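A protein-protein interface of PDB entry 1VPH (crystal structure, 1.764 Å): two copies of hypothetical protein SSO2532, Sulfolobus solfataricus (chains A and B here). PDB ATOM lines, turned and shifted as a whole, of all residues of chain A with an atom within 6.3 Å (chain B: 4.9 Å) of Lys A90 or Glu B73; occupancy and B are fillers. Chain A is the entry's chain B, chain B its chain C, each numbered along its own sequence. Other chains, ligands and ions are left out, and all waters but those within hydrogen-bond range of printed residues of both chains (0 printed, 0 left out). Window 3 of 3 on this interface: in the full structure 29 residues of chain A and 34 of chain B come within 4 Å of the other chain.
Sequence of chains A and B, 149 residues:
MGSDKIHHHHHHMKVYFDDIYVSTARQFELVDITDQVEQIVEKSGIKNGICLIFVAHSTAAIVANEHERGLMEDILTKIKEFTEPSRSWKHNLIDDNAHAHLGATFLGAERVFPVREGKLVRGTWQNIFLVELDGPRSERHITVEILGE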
ATOM      1  N   SER A  88       7.152 -10.669 -21.033  1.00  0.00           N
ATOM      2  CA  SER A  88       8.262 -11.293 -20.292  1.00  0.00           C
ATOM      3  C   SER A  88       8.034 -12.782 -20.126  1.00  0.00           C
ATOM      4  O   SER A  88       7.946 -13.314 -19.018  1.00  0.00           O
ATOM      5  CB  SER A  88       8.504 -10.597 -18.946  1.00  0.00           C
ATOM      6  OG  SER A  88       9.159  -9.353 -19.164  1.00  0.00           O
ATOM      7  N   TRP A  89       8.010 -13.477 -21.247  1.00  0.00           N
ATOM      8  CA  TRP A  89       7.985 -14.932 -21.255  1.00  0.00           C
ATOM      9  C   TRP A  89       9.208 -15.492 -20.544  1.00  0.00           C
ATOM     10  O   TRP A  89      10.297 -14.907 -20.609  1.00  0.00           O
ATOM     11  CB  TRP A  89       7.986 -15.385 -22.720  1.00  0.00           C
ATOM     12  CG  TRP A  89       6.760 -15.036 -23.487  1.00  0.00           C
ATOM     13  CD1 TRP A  89       6.669 -14.226 -24.569  1.00  0.00           C
ATOM     14  CD2 TRP A  89       5.464 -15.521 -23.236  1.00  0.00           C
ATOM     15  NE1 TRP A  89       5.387 -14.159 -25.000  1.00  0.00           N
ATOM     16  CE2 TRP A  89       4.612 -14.947 -24.193  1.00  0.00           C
ATOM     17  CE3 TRP A  89       4.926 -16.386 -22.279  1.00  0.00           C
ATOM     18  CZ2 TRP A  89       3.248 -15.265 -24.261  1.00  0.00           C
ATOM     19  CZ3 TRP A  89       3.586 -16.646 -22.308  1.00  0.00           C
ATOM     20  CH2 TRP A  89       2.761 -16.088 -23.289  1.00  0.00           C
ATOM     21  N   LYS A  90       9.051 -16.639 -19.898  1.00  0.00           N
ATOM     22  CA  LYS A  90      10.144 -17.233 -19.143  1.00  0.00           C
ATOM     23  C   LYS A  90      11.336 -17.585 -20.033  1.00  0.00           C
ATOM     24  O   LYS A  90      12.474 -17.419 -19.628  1.00  0.00           O
ATOM     25  CB  LYS A  90       9.677 -18.463 -18.354  1.00  0.00           C
ATOM     26  CG  LYS A  90       8.608 -18.160 -17.296  1.00  0.00           C
ATOM     27  CD  LYS A  90       8.067 -19.464 -16.668  1.00  0.00           C
ATOM     28  CE  LYS A  90       6.735 -19.253 -15.943  1.00  0.00           C
ATOM     29  N   HIS A  91      11.078 -18.017 -21.265  1.00  0.00           N
ATOM     30  CA  HIS A  91      12.162 -18.358 -22.176  1.00  0.00           C
ATOM     31  C   HIS A  91      13.013 -17.159 -22.526  1.00  0.00           C
ATOM     32  O   HIS A  91      14.159 -17.304 -22.933  1.00  0.00           O
ATOM     33  CB  HIS A  91      11.597 -18.894 -23.453  1.00  0.00           C
ATOM     34  CG  HIS A  91      12.643 -19.230 -24.470  1.00  0.00           C
ATOM     35  ND1 HIS A  91      13.577 -20.222 -24.271  1.00  0.00           N
ATOM     36  CD2 HIS A  91      12.925 -18.679 -25.676  1.00  0.00           C
ATOM     37  CE1 HIS A  91      14.365 -20.301 -25.335  1.00  0.00           C
ATOM     38  NE2 HIS A  91      14.008 -19.362 -26.196  1.00  0.00           N
ATOM     39  N   ASN A  92      12.461 -15.955 -22.360  1.00  0.00           N
ATOM     40  CA  ASN A  92      13.208 -14.792 -22.792  1.00  0.00           C
ATOM     41  C   ASN A  92      14.382 -14.498 -21.880  1.00  0.00           C
ATOM     42  O   ASN A  92      15.193 -13.660 -22.258  1.00  0.00           O
ATOM     43  CB  ASN A  92      12.340 -13.545 -22.940  1.00  0.00           C
ATOM     44  CG  ASN A  92      11.356 -13.659 -24.095  1.00  0.00           C
ATOM     45  OD1 ASN A  92      11.547 -14.479 -24.995  1.00  0.00           O
ATOM     46  ND2 ASN A  92      10.310 -12.833 -24.065  1.00  0.00           N
ATOM     47  N   LEU A  93      14.451 -15.134 -20.708  1.00  0.00           N
ATOM     48  CA  LEU A  93      15.670 -15.082 -19.865  1.00  0.00           C
ATOM     49  C   LEU A  93      16.867 -15.559 -20.695  1.00  0.00           C
ATOM     50  O   LEU A  93      17.981 -15.082 -20.541  1.00  0.00           O
ATOM     51  CB  LEU A  93      15.595 -15.965 -18.626  1.00  0.00           C
ATOM     52  CG  LEU A  93      14.538 -15.615 -17.588  1.00  0.00           C
ATOM     53  CD1 LEU A  93      14.586 -16.606 -16.413  1.00  0.00           C
ATOM     54  CD2 LEU A  93      14.636 -14.170 -17.127  1.00  0.00           C
ATOM     55  N   ILE A  94      16.614 -16.535 -21.574  1.00  0.00           N
ATOM     56  CA  ILE A  94      17.669 -17.151 -22.370  1.00  0.00           C
ATOM     57  C   ILE A  94      17.866 -16.487 -23.754  1.00  0.00           C
ATOM     58  O   ILE A  94      18.973 -16.147 -24.120  1.00  0.00           O
ATOM     59  CB  ILE A  94      17.406 -18.632 -22.634  1.00  0.00           C
ATOM     60  CG1 ILE A  94      17.496 -19.399 -21.324  1.00  0.00           C
ATOM     61  CG2 ILE A  94      18.407 -19.175 -23.641  1.00  0.00           C
ATOM     62  CD1 ILE A  94      17.126 -20.801 -21.465  1.00  0.00           C
ATOM     63  N   ALA A  98      10.845 -15.931 -27.388  1.00  0.00           N
ATOM     64  CA  ALA A  98       9.758 -16.822 -26.972  1.00  0.00           C
ATOM     65  C   ALA A  98       8.512 -16.682 -27.891  1.00  0.00           C
ATOM     66  O   ALA A  98       7.931 -17.665 -28.239  1.00  0.00           O
ATOM     67  CB  ALA A  98       9.346 -16.586 -25.542  1.00  0.00           C
ATOM     68  N   ARG B  69      13.001 -25.306 -20.534  1.00  0.00           N
ATOM     69  CA  ARG B  69      11.978 -25.429 -19.507  1.00  0.00           C
ATOM     70  C   ARG B  69      11.124 -24.164 -19.394  1.00  0.00           C
ATOM     71  O   ARG B  69       9.900 -24.258 -19.232  1.00  0.00           O
ATOM     72  CB  ARG B  69      12.660 -25.809 -18.149  1.00  0.00           C
ATOM     73  CG  ARG B  69      11.718 -25.758 -16.983  1.00  0.00           C
ATOM     74  CD  ARG B  69      12.351 -26.276 -15.694  1.00  0.00           C
ATOM     75  NE  ARG B  69      11.756 -25.614 -14.543  1.00  0.00           N
ATOM     76  N   GLY B  70      11.749 -22.999 -19.537  1.00  0.00           N
ATOM     77  CA  GLY B  70      11.006 -21.725 -19.571  1.00  0.00           C
ATOM     78  C   GLY B  70       9.995 -21.659 -20.709  1.00  0.00           C
ATOM     79  O   GLY B  70       8.805 -21.352 -20.497  1.00  0.00           O
ATOM     80  N   LEU B  71      10.451 -21.978 -21.919  1.00  0.00           N
ATOM     81  CA  LEU B  71       9.608 -22.033 -23.078  1.00  0.00           C
ATOM     82  C   LEU B  71       8.457 -23.012 -22.946  1.00  0.00           C
ATOM     83  O   LEU B  71       7.335 -22.777 -23.386  1.00  0.00           O
ATOM     84  CB  LEU B  71      10.441 -22.498 -24.250  1.00  0.00           C
ATOM     85  CG  LEU B  71       9.675 -22.411 -25.552  1.00  0.00           C
ATOM     86  CD1 LEU B  71       9.137 -21.005 -25.800  1.00  0.00           C
ATOM     87  CD2 LEU B  71      10.639 -22.836 -26.658  1.00  0.00           C
ATOM     88  N   MET B  72       8.749 -24.152 -22.368  1.00  0.00           N
ATOM     89  CA  MET B  72       7.707 -25.147 -22.200  1.00  0.00           C
ATOM     90  C   MET B  72       6.597 -24.566 -21.317  1.00  0.00           C
ATOM     91  O   MET B  72       5.408 -24.796 -21.550  1.00  0.00           O
ATOM     92  CB  MET B  72       8.286 -26.439 -21.617  1.00  0.00           C
ATOM     93  CG  MET B  72       9.052 -27.215 -22.634  1.00  0.00           C
ATOM     94  SD  MET B  72      10.185 -28.444 -22.000  1.00  0.00           S
ATOM     95  CE  MET B  72       9.005 -29.745 -21.538  1.00  0.00           C
ATOM     96  N   GLU B  73       6.990 -23.839 -20.284  1.00  0.00           N
ATOM     97  CA  GLU B  73       6.029 -23.178 -19.429  1.00  0.00           C
ATOM     98  C   GLU B  73       5.273 -22.082 -20.214  1.00  0.00           C
ATOM     99  O   GLU B  73       4.067 -21.983 -20.053  1.00  0.00           O
ATOM    100  CB  GLU B  73       6.696 -22.675 -18.145  1.00  0.00           C
ATOM    101  CG  GLU B  73       6.955 -23.799 -17.179  1.00  0.00           C
ATOM    102  CD  GLU B  73       7.702 -23.345 -15.921  1.00  0.00           C
ATOM    103  OE1 GLU B  73       7.634 -22.132 -15.586  1.00  0.00           O
ATOM    104  OE2 GLU B  73       8.356 -24.207 -15.276  1.00  0.00           O
ATOM    105  N   ASP B  74       5.974 -21.293 -21.042  1.00  0.00           N
ATOM    106  CA  ASP B  74       5.335 -20.279 -21.905  1.00  0.00           C
ATOM    107  C   ASP B  74       4.291 -20.911 -22.822  1.00  0.00           C
ATOM    108  O   ASP B  74       3.146 -20.440 -22.927  1.00  0.00           O
ATOM    109  CB  ASP B  74       6.383 -19.527 -22.714  1.00  0.00           C
ATOM    110  CG  ASP B  74       7.454 -18.861 -21.836  1.00  0.00           C
ATOM    111  OD1 ASP B  74       7.140 -18.373 -20.687  1.00  0.00           O
ATOM    112  OD2 ASP B  74       8.615 -18.796 -22.305  1.00  0.00           O
ATOM    113  N   ILE B  75       4.680 -21.987 -23.494  1.00  0.00           N
ATOM    114  CA  ILE B  75       3.744 -22.700 -24.375  1.00  0.00           C
ATOM    115  C   ILE B  75       2.437 -23.059 -23.667  1.00  0.00           C
ATOM    116  O   ILE B  75       1.347 -22.753 -24.158  1.00  0.00           O
ATOM    117  CB  ILE B  75       4.390 -23.960 -24.973  1.00  0.00           C
ATOM    118  CG1 ILE B  75       5.452 -23.544 -26.001  1.00  0.00           C
ATOM    119  CG2 ILE B  75       3.339 -24.781 -25.684  1.00  0.00           C
ATOM    120  CD1 ILE B  75       6.405 -24.692 -26.396  1.00  0.00           C
ATOM    121  N   LEU B  76       2.551 -23.654 -22.479  1.00  0.00           N
ATOM    122  CA  LEU B  76       1.382 -24.111 -21.752  1.00  0.00           C
ATOM    123  C   LEU B  76       0.599 -22.909 -21.216  1.00  0.00           C
ATOM    124  O   LEU B  76      -0.622 -22.968 -21.144  1.00  0.00           O
ATOM    125  CB  LEU B  76       1.790 -25.050 -20.597  1.00  0.00           C
ATOM    126  CG  LEU B  76       2.272 -26.436 -20.975  1.00  0.00           C
ATOM    127  CD1 LEU B  76       2.676 -27.211 -19.740  1.00  0.00           C
ATOM    128  CD2 LEU B  76       1.243 -27.262 -21.773  1.00  0.00           C
ATOM    129  N   THR B  77       1.305 -21.843 -20.853  1.00  0.00           N
ATOM    130  CA  THR B  77       0.644 -20.637 -20.362  1.00  0.00           C
ATOM    131  C   THR B  77      -0.193 -20.001 -21.476  1.00  0.00           C
ATOM    132  O   THR B  77      -1.349 -19.621 -21.241  1.00  0.00           O
ATOM    133  CB  THR B  77       1.655 -19.670 -19.841  1.00  0.00           C
ATOM    134  OG1 THR B  77       2.198 -20.212 -18.616  1.00  0.00           O
ATOM    135  CG2 THR B  77       0.981 -18.350 -19.557  1.00  0.00           C
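Hydrophobic or aromatic side chains of chain A that line the printed part of chain B: Trp A89, His A91 and Ala A98.
Of the 9 printed residues of chain B, 4 touch a printed residue of chain A.
Hydrophobic or aromatic side chains of chain B within 4 Å of the printed part of chain A: Leu B71.
Along chain B the printed residues that touch a printed residue of chain A span positions 70 to 74.
Among the printed residues, 8 pairs touch across the chains.
Among the printed residues, no Asp or Glu carboxylate lies within 4 Å of a Lys or Arg side-chain nitrogen of the other chain.
Of the printed residues of chain B, Trp A89 touches Asp B74.
Lys A90 touches three residues of chain B.
Of the printed residues of chain B, His A91 touches Gly B70, Leu B71 and Asp B74.
Printed residues of chain B within 4 Å of Ala A98: Asp B74 (3.99 Å).
Printed residues of chain A within 4 Å of Gly B70: Lys A90 and His A91.
Of the printed residues of chain A, Glu B73 touches Lys A90 (2.9 Å).
Printed residues of chain A within 4 Å of Asp B74: Trp A89 (3.4 Å), Lys A90 (2.7 Å), His A91 (2.8 Å) and Ala A98 (3.99 Å).
Ile B75 touches none of the printed residues of chain A.
Leu B76 touches none of the printed residues of chain A.
The nearest printed residue of chain B that does not touch Lys A90 is Leu B71 (4.9 Å).
N of Ala A98 lies within hydrogen-bond range of OD1 of Asn A92 (2.9 Å).
The guanidinium group (NE) of Arg B69 lies within salt-bridge range of the side-chain carboxylate (OE2) of Glu B73 (3.8 Å).
O of Glu B73 sits at hydrogen-bond distance from OG1 of Thr B77 (2.9 Å).
CE3 of Trp A89 touches OD1 of Asp B74, at 3.4 Å.
Gly B70 touches Lys A90.
Glu B73 touches Lys A90.
His A91 touches Gly B70 (N to C, 3.8 Å).
N of Leu B71 touches CB of His A91, 3.6 Å away.
CB of Ala A98 touches OD2 of Asp B74 (3.99 Å).
No position is printed for both chains.
The backbone NH of His A91 lies within hydrogen-bond range of the side-chain carboxylate of Asp B74, at 2.8 Å.
The side-chain carboxylate (OD1) of Asp B74 lies within hydrogen-bond range of the backbone NH (N) of Lys A90 (2.7 Å).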
